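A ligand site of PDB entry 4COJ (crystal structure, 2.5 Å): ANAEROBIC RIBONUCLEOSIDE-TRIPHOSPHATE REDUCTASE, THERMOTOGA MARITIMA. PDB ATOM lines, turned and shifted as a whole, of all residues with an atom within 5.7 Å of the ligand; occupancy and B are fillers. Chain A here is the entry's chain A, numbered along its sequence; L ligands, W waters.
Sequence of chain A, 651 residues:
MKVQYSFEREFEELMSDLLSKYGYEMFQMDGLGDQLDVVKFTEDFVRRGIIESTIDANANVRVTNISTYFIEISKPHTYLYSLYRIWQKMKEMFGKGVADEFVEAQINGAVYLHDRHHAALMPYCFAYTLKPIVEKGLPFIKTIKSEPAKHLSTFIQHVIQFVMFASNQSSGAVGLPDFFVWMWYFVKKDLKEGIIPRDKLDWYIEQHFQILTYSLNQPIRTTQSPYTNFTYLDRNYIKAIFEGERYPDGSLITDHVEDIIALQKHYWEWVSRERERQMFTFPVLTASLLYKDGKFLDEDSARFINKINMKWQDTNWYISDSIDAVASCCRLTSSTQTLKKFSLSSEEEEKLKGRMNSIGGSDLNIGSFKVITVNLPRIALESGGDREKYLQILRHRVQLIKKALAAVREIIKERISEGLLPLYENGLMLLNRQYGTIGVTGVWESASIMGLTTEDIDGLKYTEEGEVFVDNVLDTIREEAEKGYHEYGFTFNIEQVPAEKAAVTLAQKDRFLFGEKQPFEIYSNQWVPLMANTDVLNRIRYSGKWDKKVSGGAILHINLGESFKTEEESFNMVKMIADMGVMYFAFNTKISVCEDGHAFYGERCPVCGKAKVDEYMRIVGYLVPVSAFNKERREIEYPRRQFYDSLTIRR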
ATOM      1  N   TYR A 112      -0.425 -21.684  -8.742  1.00  0.00           N
ATOM      2  CA  TYR A 112       0.838 -22.197  -8.220  1.00  0.00           C
ATOM      3  C   TYR A 112       1.715 -21.048  -7.749  1.00  0.00           C
ATOM      4  O   TYR A 112       2.266 -20.305  -8.553  1.00  0.00           O
ATOM      5  CB  TYR A 112       1.571 -23.022  -9.276  1.00  0.00           C
ATOM      6  CG  TYR A 112       2.758 -23.779  -8.727  1.00  0.00           C
ATOM      7  CD1 TYR A 112       4.011 -23.175  -8.637  1.00  0.00           C
ATOM      8  CD2 TYR A 112       2.629 -25.082  -8.286  1.00  0.00           C
ATOM      9  CE1 TYR A 112       5.091 -23.859  -8.123  1.00  0.00           C
ATOM     10  CE2 TYR A 112       3.710 -25.785  -7.780  1.00  0.00           C
ATOM     11  CZ  TYR A 112       4.930 -25.168  -7.700  1.00  0.00           C
ATOM     12  OH  TYR A 112       6.010 -25.861  -7.190  1.00  0.00           O
ATOM     13  N   LEU A 113       1.826 -20.911  -6.438  1.00  0.00           N
ATOM     14  CA  LEU A 113       2.784 -19.987  -5.835  1.00  0.00           C
ATOM     15  C   LEU A 113       4.188 -20.558  -6.005  1.00  0.00           C
ATOM     16  O   LEU A 113       4.471 -21.684  -5.590  1.00  0.00           O
ATOM     17  CB  LEU A 113       2.463 -19.773  -4.356  1.00  0.00           C
ATOM     18  CG  LEU A 113       3.322 -18.759  -3.596  1.00  0.00           C
ATOM     19  CD1 LEU A 113       3.077 -17.349  -4.111  1.00  0.00           C
ATOM     20  CD2 LEU A 113       3.050 -18.821  -2.098  1.00  0.00           C
ATOM     21  N   HIS A 114       5.059 -19.782  -6.633  1.00  0.00           N
ATOM     22  CA  HIS A 114       6.425 -20.251  -6.897  1.00  0.00           C
ATOM     23  C   HIS A 114       7.350 -19.950  -5.726  1.00  0.00           C
ATOM     24  O   HIS A 114       7.216 -18.938  -5.051  1.00  0.00           O
ATOM     25  CB  HIS A 114       6.954 -19.605  -8.166  1.00  0.00           C
ATOM     26  CG  HIS A 114       6.367 -20.177  -9.421  1.00  0.00           C
ATOM     27  ND1 HIS A 114       6.783 -21.381  -9.959  1.00  0.00           N
ATOM     28  CD2 HIS A 114       5.384 -19.732 -10.229  1.00  0.00           C
ATOM     29  CE1 HIS A 114       6.090 -21.636 -11.050  1.00  0.00           C
ATOM     30  NE2 HIS A 114       5.229 -20.654 -11.235  1.00  0.00           N
ATOM     31  N   ASP A 115       8.307 -20.859  -5.521  1.00  0.00           N
ATOM     32  CA  ASP A 115       9.225 -20.782  -4.386  1.00  0.00           C
ATOM     33  C   ASP A 115       8.461 -20.460  -3.099  1.00  0.00           C
ATOM     34  O   ASP A 115       8.835 -19.572  -2.341  1.00  0.00           O
ATOM     35  CB  ASP A 115      10.315 -19.737  -4.642  1.00  0.00           C
ATOM     36  CG  ASP A 115      11.016 -19.954  -5.982  1.00  0.00           C
ATOM     37  OD1 ASP A 115      11.776 -20.942  -6.108  1.00  0.00           O
ATOM     38  OD2 ASP A 115      10.801 -19.129  -6.909  1.00  0.00           O
ATOM     39  N   ARG A 116       7.390 -21.210  -2.869  1.00  0.00           N
ATOM     40  CA  ARG A 116       6.449 -20.893  -1.800  1.00  0.00           C
ATOM     41  C   ARG A 116       7.099 -20.970  -0.417  1.00  0.00           C
ATOM     42  O   ARG A 116       6.712 -20.237   0.494  1.00  0.00           O
ATOM     43  CB  ARG A 116       5.253 -21.831  -1.863  1.00  0.00           C
ATOM     44  CG  ARG A 116       5.583 -23.303  -1.754  1.00  0.00           C
ATOM     45  CD  ARG A 116       4.460 -24.142  -2.299  1.00  0.00           C
ATOM     46  NE  ARG A 116       4.593 -25.556  -1.970  1.00  0.00           N
ATOM     47  CZ  ARG A 116       5.253 -26.444  -2.707  1.00  0.00           C
ATOM     48  NH1 ARG A 116       5.850 -26.070  -3.838  1.00  0.00           N
ATOM     49  NH2 ARG A 116       5.314 -27.701  -2.321  1.00  0.00           N
ATOM     50  N   HIS A 117       8.081 -21.839  -0.278  1.00  0.00           N
ATOM     51  CA  HIS A 117       8.862 -21.929   0.950  1.00  0.00           C
ATOM     52  C   HIS A 117       9.649 -20.632   1.236  1.00  0.00           C
ATOM     53  O   HIS A 117      10.099 -20.427   2.359  1.00  0.00           O
ATOM     54  CB  HIS A 117       9.824 -23.129   0.892  1.00  0.00           C
ATOM     55  CG  HIS A 117      10.684 -23.168  -0.332  1.00  0.00           C
ATOM     56  ND1 HIS A 117      10.189 -23.428  -1.589  1.00  0.00           N
ATOM     57  CD2 HIS A 117      12.024 -22.987  -0.489  1.00  0.00           C
ATOM     58  CE1 HIS A 117      11.168 -23.408  -2.472  1.00  0.00           C
ATOM     59  NE2 HIS A 117      12.290 -23.146  -1.823  1.00  0.00           N
ATOM     60  N   TYR A 124      12.496 -13.148  -5.790  1.00  0.00           N
ATOM     61  CA  TYR A 124      12.708 -14.233  -6.742  1.00  0.00           C
ATOM     62  C   TYR A 124      13.997 -14.075  -7.547  1.00  0.00           C
ATOM     63  O   TYR A 124      14.947 -14.811  -7.314  1.00  0.00           O
ATOM     64  CB  TYR A 124      11.475 -14.334  -7.633  1.00  0.00           C
ATOM     65  CG  TYR A 124      11.614 -15.119  -8.920  1.00  0.00           C
ATOM     66  CD1 TYR A 124      12.086 -16.420  -8.938  1.00  0.00           C
ATOM     67  CD2 TYR A 124      11.225 -14.557 -10.127  1.00  0.00           C
ATOM     68  CE1 TYR A 124      12.182 -17.133 -10.120  1.00  0.00           C
ATOM     69  CE2 TYR A 124      11.318 -15.246 -11.311  1.00  0.00           C
ATOM     70  CZ  TYR A 124      11.793 -16.546 -11.306  1.00  0.00           C
ATOM     71  OH  TYR A 124      11.884 -17.223 -12.495  1.00  0.00           O
ATOM     72  N   CYS A 125      14.042 -13.124  -8.478  1.00  0.00           N
ATOM     73  CA  CYS A 125      15.224 -12.993  -9.338  1.00  0.00           C
ATOM     74  C   CYS A 125      15.456 -11.586  -9.879  1.00  0.00           C
ATOM     75  O   CYS A 125      14.546 -10.755  -9.918  1.00  0.00           O
ATOM     76  CB  CYS A 125      15.110 -13.969 -10.518  1.00  0.00           C
ATOM     77  SG  CYS A 125      14.043 -13.391 -11.860  1.00  0.00           S
ATOM     78  N   SER A 171      15.408 -16.535  -4.560  1.00  0.00           N
ATOM     79  CA  SER A 171      15.080 -17.888  -4.957  1.00  0.00           C
ATOM     80  C   SER A 171      15.496 -18.226  -6.385  1.00  0.00           C
ATOM     81  O   SER A 171      15.748 -19.391  -6.707  1.00  0.00           O
ATOM     82  CB  SER A 171      13.579 -18.106  -4.813  1.00  0.00           C
ATOM     83  OG  SER A 171      13.173 -17.768  -3.509  1.00  0.00           O
ATOM     84  N   GLY A 172      15.555 -17.210  -7.237  1.00  0.00           N
ATOM     85  CA  GLY A 172      15.688 -17.412  -8.670  1.00  0.00           C
ATOM     86  C   GLY A 172      17.065 -17.078  -9.235  1.00  0.00           C
ATOM     87  O   GLY A 172      18.073 -17.137  -8.538  1.00  0.00           O
ATOM     88  N   ALA A 173      17.079 -16.721 -10.513  1.00  0.00           N
ATOM     89  CA  ALA A 173      18.316 -16.525 -11.236  1.00  0.00           C
ATOM     90  C   ALA A 173      19.078 -15.313 -10.726  1.00  0.00           C
ATOM     91  O   ALA A 173      18.487 -14.340 -10.256  1.00  0.00           O
ATOM     92  CB  ALA A 173      18.036 -16.361 -12.718  1.00  0.00           C
ATOM     93  N   ARG A 221      24.324 -22.948  -3.276  1.00  0.00           N
ATOM     94  CA  ARG A 221      23.011 -22.956  -2.624  1.00  0.00           C
ATOM     95  C   ARG A 221      22.814 -24.263  -1.851  1.00  0.00           C
ATOM     96  O   ARG A 221      21.680 -24.706  -1.636  1.00  0.00           O
ATOM     97  CB  ARG A 221      21.880 -22.762  -3.658  1.00  0.00           C
ATOM     98  CG  ARG A 221      21.863 -21.364  -4.293  1.00  0.00           C
ATOM     99  CD  ARG A 221      20.606 -21.130  -5.130  1.00  0.00           C
ATOM    100  NE  ARG A 221      20.501 -22.092  -6.240  1.00  0.00           N
ATOM    101  CZ  ARG A 221      19.559 -22.056  -7.181  1.00  0.00           C
ATOM    102  NH1 ARG A 221      18.640 -21.103  -7.177  1.00  0.00           N
ATOM    103  NH2 ARG A 221      19.546 -22.982  -8.130  1.00  0.00           N
ATOM    104  N   GLN A 224      22.304 -27.343  -4.260  1.00  0.00           N
ATOM    105  CA  GLN A 224      22.653 -27.224  -5.674  1.00  0.00           C
ATOM    106  C   GLN A 224      23.469 -25.964  -5.937  1.00  0.00           C
ATOM    107  O   GLN A 224      23.683 -25.148  -5.032  1.00  0.00           O
ATOM    108  CB  GLN A 224      21.400 -27.208  -6.534  1.00  0.00           C
ATOM    109  CG  GLN A 224      20.499 -25.993  -6.273  1.00  0.00           C
ATOM    110  CD  GLN A 224      19.124 -26.137  -6.876  1.00  0.00           C
ATOM    111  OE1 GLN A 224      18.924 -26.886  -7.834  1.00  0.00           O
ATOM    112  NE2 GLN A 224      18.153 -25.425  -6.311  1.00  0.00           N
ATOM    113  N   SER A 225      23.915 -25.816  -7.173  1.00  0.00           N
ATOM    114  CA  SER A 225      24.626 -24.615  -7.571  1.00  0.00           C
ATOM    115  C   SER A 225      23.656 -23.464  -7.784  1.00  0.00           C
ATOM    116  O   SER A 225      22.456 -23.689  -7.940  1.00  0.00           O
ATOM    117  CB  SER A 225      25.435 -24.867  -8.838  1.00  0.00           C
ATOM    118  OG  SER A 225      24.692 -25.635  -9.754  1.00  0.00           O
ATOM    119  N   TYR A 227      21.718 -20.465  -9.810  1.00  0.00           N
ATOM    120  CA  TYR A 227      21.267 -20.327 -11.177  1.00  0.00           C
ATOM    121  C   TYR A 227      21.756 -18.983 -11.689  1.00  0.00           C
ATOM    122  O   TYR A 227      21.346 -17.932 -11.171  1.00  0.00           O
ATOM    123  CB  TYR A 227      19.744 -20.426 -11.267  1.00  0.00           C
ATOM    124  CG  TYR A 227      19.239 -20.575 -12.685  1.00  0.00           C
ATOM    125  CD1 TYR A 227      19.196 -19.487 -13.541  1.00  0.00           C
ATOM    126  CD2 TYR A 227      18.822 -21.805 -13.155  1.00  0.00           C
ATOM    127  CE1 TYR A 227      18.750 -19.620 -14.833  1.00  0.00           C
ATOM    128  CE2 TYR A 227      18.368 -21.957 -14.454  1.00  0.00           C
ATOM    129  CZ  TYR A 227      18.327 -20.859 -15.284  1.00  0.00           C
ATOM    130  OH  TYR A 227      17.872 -21.002 -16.578  1.00  0.00           O
ATOM    131  N   PHE A 282      26.007 -24.212 -15.808  1.00  0.00           N
ATOM    132  CA  PHE A 282      26.008 -22.765 -15.656  1.00  0.00           C
ATOM    133  C   PHE A 282      27.345 -22.146 -16.052  1.00  0.00           C
ATOM    134  O   PHE A 282      28.362 -22.833 -16.054  1.00  0.00           O
ATOM    135  CB  PHE A 282      25.664 -22.401 -14.200  1.00  0.00           C
ATOM    136  CG  PHE A 282      24.325 -22.883 -13.770  1.00  0.00           C
ATOM    137  CD1 PHE A 282      23.173 -22.273 -14.221  1.00  0.00           C
ATOM    138  CD2 PHE A 282      24.214 -23.960 -12.909  1.00  0.00           C
ATOM    139  CE1 PHE A 282      21.926 -22.721 -13.830  1.00  0.00           C
ATOM    140  CE2 PHE A 282      22.969 -24.412 -12.509  1.00  0.00           C
ATOM    141  CZ  PHE A 282      21.827 -23.801 -12.962  1.00  0.00           C
ATOM    142  N   SER A 358      12.481 -16.087 -17.334  1.00  0.00           N
ATOM    143  CA  SER A 358      12.965 -16.834 -16.191  1.00  0.00           C
ATOM    144  C   SER A 358      14.182 -17.686 -16.546  1.00  0.00           C
ATOM    145  O   SER A 358      15.120 -17.799 -15.757  1.00  0.00           O
ATOM    146  CB  SER A 358      11.854 -17.704 -15.605  1.00  0.00           C
ATOM    147  OG  SER A 358      10.839 -16.894 -15.045  1.00  0.00           O
ATOM    148  N   ILE A 359      14.151 -18.294 -17.736  1.00  0.00           N
ATOM    149  CA  ILE A 359      15.231 -19.157 -18.188  1.00  0.00           C
ATOM    150  C   ILE A 359      16.516 -18.371 -18.394  1.00  0.00           C
ATOM    151  O   ILE A 359      17.583 -18.760 -17.911  1.00  0.00           O
ATOM    152  CB  ILE A 359      14.855 -19.861 -19.509  1.00  0.00           C
ATOM    153  CG1 ILE A 359      13.700 -20.826 -19.272  1.00  0.00           C
ATOM    154  CG2 ILE A 359      16.061 -20.620 -20.111  1.00  0.00           C
ATOM    155  CD1 ILE A 359      12.954 -21.198 -20.532  1.00  0.00           C
ATOM    156  N   GLY A 360      16.409 -17.257 -19.116  1.00  0.00           N
ATOM    157  CA  GLY A 360      17.554 -16.455 -19.483  1.00  0.00           C
ATOM    158  C   GLY A 360      17.161 -15.427 -20.531  1.00  0.00           C
ATOM    159  O   GLY A 360      16.113 -15.547 -21.172  1.00  0.00           O
ATOM    160  N   VAL A 497       5.863 -20.122 -17.982  1.00  0.00           N
ATOM    161  CA  VAL A 497       6.973 -20.551 -17.139  1.00  0.00           C
ATOM    162  C   VAL A 497       7.457 -21.956 -17.477  1.00  0.00           C
ATOM    163  O   VAL A 497       6.708 -22.761 -18.021  1.00  0.00           O
ATOM    164  CB  VAL A 497       6.571 -20.497 -15.654  1.00  0.00           C
ATOM    165  CG1 VAL A 497       6.217 -19.070 -15.248  1.00  0.00           C
ATOM    166  CG2 VAL A 497       5.402 -21.433 -15.359  1.00  0.00           C
ATOM    167  N   PRO A 498       8.732 -22.253 -17.155  1.00  0.00           N
ATOM    168  CA  PRO A 498       9.281 -23.600 -17.361  1.00  0.00           C
ATOM    169  C   PRO A 498       8.508 -24.672 -16.611  1.00  0.00           C
ATOM    170  O   PRO A 498       8.401 -25.797 -17.104  1.00  0.00           O
ATOM    171  CB  PRO A 498      10.720 -23.487 -16.829  1.00  0.00           C
ATOM    172  CG  PRO A 498      11.039 -22.046 -16.924  1.00  0.00           C
ATOM    173  CD  PRO A 498       9.758 -21.334 -16.634  1.00  0.00           C
ATOM    174  N   ALA A 499       7.977 -24.319 -15.439  1.00  0.00           N
ATOM    175  CA  ALA A 499       7.137 -25.222 -14.660  1.00  0.00           C
ATOM    176  C   ALA A 499       7.780 -26.583 -14.485  1.00  0.00           C
ATOM    177  O   ALA A 499       7.194 -27.616 -14.827  1.00  0.00           O
ATOM    178  CB  ALA A 499       5.766 -25.363 -15.295  1.00  0.00           C
ATOM    179  N   GLU A 500       9.006 -26.592 -13.979  1.00  0.00           N
ATOM    180  CA  GLU A 500       9.761 -27.826 -13.830  1.00  0.00           C
ATOM    181  C   GLU A 500       9.068 -28.760 -12.854  1.00  0.00           C
ATOM    182  O   GLU A 500       9.118 -29.974 -13.009  1.00  0.00           O
ATOM    183  CB  GLU A 500      11.183 -27.511 -13.366  1.00  0.00           C
ATOM    184  CG  GLU A 500      12.099 -28.717 -13.340  1.00  0.00           C
ATOM    185  CD  GLU A 500      13.527 -28.353 -12.989  1.00  0.00           C
ATOM    186  OE1 GLU A 500      13.905 -27.173 -13.181  1.00  0.00           O
ATOM    187  OE2 GLU A 500      14.269 -29.245 -12.522  1.00  0.00           O
ATOM    188  N   LYS A 501       8.410 -28.181 -11.848  1.00  0.00           N
ATOM    189  CA  LYS A 501       7.681 -28.956 -10.842  1.00  0.00           C
ATOM    190  C   LYS A 501       6.166 -28.752 -10.953  1.00  0.00           C
ATOM    191  O   LYS A 501       5.393 -29.709 -10.882  1.00  0.00           O
ATOM    192  CB  LYS A 501       8.157 -28.590  -9.428  1.00  0.00           C
ATOM    193  CG  LYS A 501       9.590 -29.024  -9.119  1.00  0.00           C
ATOM    194  CD  LYS A 501       9.965 -28.769  -7.662  1.00  0.00           C
ATOM    195  CE  LYS A 501      10.267 -27.305  -7.402  1.00  0.00           C
ATOM    196  NZ  LYS A 501      11.603 -26.901  -7.907  1.00  0.00           N
ATOM    197  N   ALA A 502       5.759 -27.499 -11.145  1.00  0.00           N
ATOM    198  CA  ALA A 502       4.336 -27.148 -11.204  1.00  0.00           C
ATOM    199  C   ALA A 502       3.614 -27.910 -12.310  1.00  0.00           C
ATOM    200  O   ALA A 502       2.427 -28.217 -12.193  1.00  0.00           O
ATOM    201  CB  ALA A 502       4.182 -25.657 -11.409  1.00  0.00           C
ATOM    202  N   ALA A 503       4.318 -28.224 -13.393  1.00  0.00           N
ATOM    203  CA  ALA A 503       3.723 -28.955 -14.502  1.00  0.00           C
ATOM    204  C   ALA A 503       3.268 -30.350 -14.073  1.00  0.00           C
ATOM    205  O   ALA A 503       2.428 -30.975 -14.722  1.00  0.00           O
ATOM    206  CB  ALA A 503       4.717 -29.062 -15.650  1.00  0.00           C
ATOM    207  N   TYR A 622      17.174 -24.831 -20.124  1.00  0.00           N
ATOM    208  CA  TYR A 622      18.607 -24.876 -19.887  1.00  0.00           C
ATOM    209  C   TYR A 622      19.093 -26.319 -19.800  1.00  0.00           C
ATOM    210  O   TYR A 622      18.315 -27.224 -19.520  1.00  0.00           O
ATOM    211  CB  TYR A 622      18.969 -24.104 -18.601  1.00  0.00           C
ATOM    212  CG  TYR A 622      18.413 -24.698 -17.327  1.00  0.00           C
ATOM    213  CD1 TYR A 622      17.040 -24.818 -17.138  1.00  0.00           C
ATOM    214  CD2 TYR A 622      19.253 -25.119 -16.313  1.00  0.00           C
ATOM    215  CE1 TYR A 622      16.531 -25.363 -15.975  1.00  0.00           C
ATOM    216  CE2 TYR A 622      18.744 -25.654 -15.146  1.00  0.00           C
ATOM    217  CZ  TYR A 622      17.377 -25.775 -14.980  1.00  0.00           C
ATOM    218  OH  TYR A 622      16.854 -26.305 -13.830  1.00  0.00           O
HETATM  219  N1  LIG L   1      15.460 -21.920 -10.976  1.00  0.00           N
HETATM  220  C1  LIG L   1      16.508 -21.915 -10.040  1.00  0.00           C
HETATM  221  N2  LIG L   1      17.223 -23.046  -9.808  1.00  0.00           N
HETATM  222  C2  LIG L   1      16.945 -24.182 -10.479  1.00  0.00           C
HETATM  223  C3  LIG L   1      15.909 -24.199 -11.410  1.00  0.00           C
HETATM  224  C4  LIG L   1      15.172 -23.049 -11.641  1.00  0.00           C
HETATM  225  O1  LIG L   1      16.791 -20.870  -9.408  1.00  0.00           O
HETATM  226  N3  LIG L   1      17.657 -25.300 -10.252  1.00  0.00           N
HETATM  227  C5  LIG L   1      14.678 -20.711 -11.249  1.00  0.00           C
HETATM  228  C6  LIG L   1      15.188 -20.101 -12.540  1.00  0.00           C
HETATM  229  O2  LIG L   1      15.145 -18.661 -12.481  1.00  0.00           O
HETATM  230  C7  LIG L   1      14.231 -20.630 -13.588  1.00  0.00           C
HETATM  231  C8  LIG L   1      12.937 -20.781 -12.801  1.00  0.00           C
HETATM  232  O3  LIG L   1      13.302 -21.058 -11.450  1.00  0.00           O
HETATM  233  O4  LIG L   1      14.073 -19.758 -14.695  1.00  0.00           O
HETATM  234  C9  LIG L   1      12.054 -21.890 -13.342  1.00  0.00           C
HETATM  235  O5  LIG L   1      11.240 -22.310 -12.261  1.00  0.00           O
HETATM  236  P1  LIG L   1      10.023 -23.321 -12.514  1.00  0.00           P
HETATM  237  O6  LIG L   1      10.570 -24.627 -13.023  1.00  0.00           O
HETATM  238  O7  LIG L   1       8.979 -22.573 -13.329  1.00  0.00           O
HETATM  239  O8  LIG L   1       9.493 -23.495 -10.996  1.00  0.00           O
HETATM  240  P2  LIG L   1       8.848 -24.854 -10.446  1.00  0.00           P
HETATM  241  O9  LIG L   1       9.948 -25.844 -10.183  1.00  0.00           O
HETATM  242  O10 LIG L   1       7.685 -25.239 -11.325  1.00  0.00           O
HETATM  243  O11 LIG L   1       8.226 -24.369  -9.035  1.00  0.00           O
HETATM  244  P3  LIG L   1       9.113 -23.848  -7.799  1.00  0.00           P
HETATM  245  O12 LIG L   1       8.565 -24.643  -6.642  1.00  0.00           O
HETATM  246  O13 LIG L   1       8.824 -22.377  -7.718  1.00  0.00           O
HETATM  247  O14 LIG L   1      10.541 -24.214  -8.166  1.00  0.00           O
HETATM  248  O   HOH W   1       8.986 -19.875 -12.070  1.00  0.00           O
HETATM  249  O   HOH W   2      10.903 -21.191  -9.142  1.00  0.00           O
HETATM  250  O   HOH W   3      15.039 -15.721 -13.765  1.00  0.00           O
HETATM  251  O   HOH W   4      20.883 -26.237 -10.245  1.00  0.00           O
HETATM  252  O   HOH W   5      12.402 -24.462 -10.449  1.00  0.00           O
HETATM  253  O   HOH W   6      12.981 -22.357  -8.708  1.00  0.00           O
HETATM  254  O   HOH W   7       6.466 -23.155  -4.780  1.00  0.00           O
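The backbone carbonyl oxygen (O) of Ser 358 lies within hydrogen-bond range of an oxygen (O4) of the ligand, 2.5 Å away. N of Glu 500 is in hydrogen-bond range of O6 of the ligand (2.7 Å). N of Asp 115 lies within hydrogen-bond range of O13 of the ligand (2.7 Å). A nitrogen (N2) of the ligand is in hydrogen-bond range of the guanidinium group of Arg 221. The side-chain hydroxyl (OH) of Tyr 112 lies within hydrogen-bond range of an oxygen (O12) of the ligand (2.9 Å). O10 of the ligand sits at hydrogen-bond distance from N of Lys 501 (3.1 Å). NZ of Lys 501 lies within salt-bridge range of O14 of the ligand (2.9 Å). O7 of the ligand is in hydrogen-bond range of N of Ala 499, at 2.9 Å. The backbone NH (N) of Ala 502 is in hydrogen-bond range of an oxygen (O10) of the ligand (3.0 Å). N3 of the ligand sits at hydrogen-bond distance from OE1 of Gln 224, at 3.2 Å. An oxygen (O13) of the ligand is in hydrogen-bond range of a ring nitrogen (ND1) of His 114 (3.2 Å). The backbone NH of Ala 173 lies within hydrogen-bond range of an oxygen (O2) of the ligand, 3.4 Å away. The backbone NH of Ile 359 sits at hydrogen-bond distance from an oxygen (O4) of the ligand (3.4 Å).
The side-chain hydroxyl (OG) of Ser 358 sits at hydrogen-bond distance from the side-chain hydroxyl (OH) of Tyr 124 (2.8 Å). NH2 of Arg 221 lies close to NE2 of Gln 224. O of Ser 171 sits at hydrogen-bond distance from NH1 of Arg 221 (3.4 Å). The guanidinium group (NH2) of Arg 221 sits at hydrogen-bond distance from the backbone carbonyl oxygen (O) of Ser 225 (3.0 Å). The side-chain hydroxyl (OH) of Tyr 112 is in hydrogen-bond range of the guanidinium group (NH1) of Arg 116. The backbone NH of Ser 171 is in hydrogen-bond range of the backbone carbonyl oxygen of Tyr 124 (3.3 Å). O of Ile 359 sits at hydrogen-bond distance from OH of Tyr 227 (2.6 Å). The backbone carbonyl oxygen (O) of Tyr 124 lies within hydrogen-bond range of the backbone NH (N) of Gly 172 (2.5 Å).
The backbone carbonyl oxygen (O) of Ser 171 lies close to an oxygen (O1) of the ligand (3.3 Å). Merely in contact with the ligand: Tyr 622 (3.3 Å), Tyr 227 (3.5 Å), Tyr 124 (3.6 Å), Pro 498 (3.6 Å), Gly 172 (3.7 Å) and Val 497 (3.9 Å). Hydrophobic or aromatic side chains that line the ligand: Tyr 112, His 114, Ala 173, Tyr 227, Val 497, Pro 498 and Ala 502. Within 4 Å of the ligand: Tyr 112, His 114, Asp 115, Tyr 124, Ser 171, Gly 172, Ala 173, Arg 221, Gln 224, Tyr 227, Ser 358, Ile 359, Val 497, Pro 498, Ala 499, Glu 500, Lys 501, Ala 502 and Tyr 622. The nearest printed residue that does not touch the ligand is Arg 116 (4.2 Å).
Water W2 lies within hydrogen-bond range of O13 of the ligand (2.8 Å) and OD2 of Asp 115 (3.0 Å). Water W1 lies within hydrogen-bond range of O7 of the ligand (3.0 Å) and ND1 of His 114 (3.4 Å). Water W6 lies within hydrogen-bond range of an oxygen (O3) of the ligand (3.1 Å) and the side-chain carboxylate of Asp 115 (3.2 Å). Water W7 lies within hydrogen-bond range of O of Leu 113, N of Arg 116, N of Asp 115 and O12 of the ligand. Water W3 lies within hydrogen-bond range of O of Ser 358 (2.9 Å), SG of Cys 125 (3.2 Å) and O2 of the ligand (3.2 Å). Water W4 lies within hydrogen-bond range of the side-chain amide oxygen (OE1) of Gln 224 and a nitrogen (N3) of the ligand.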
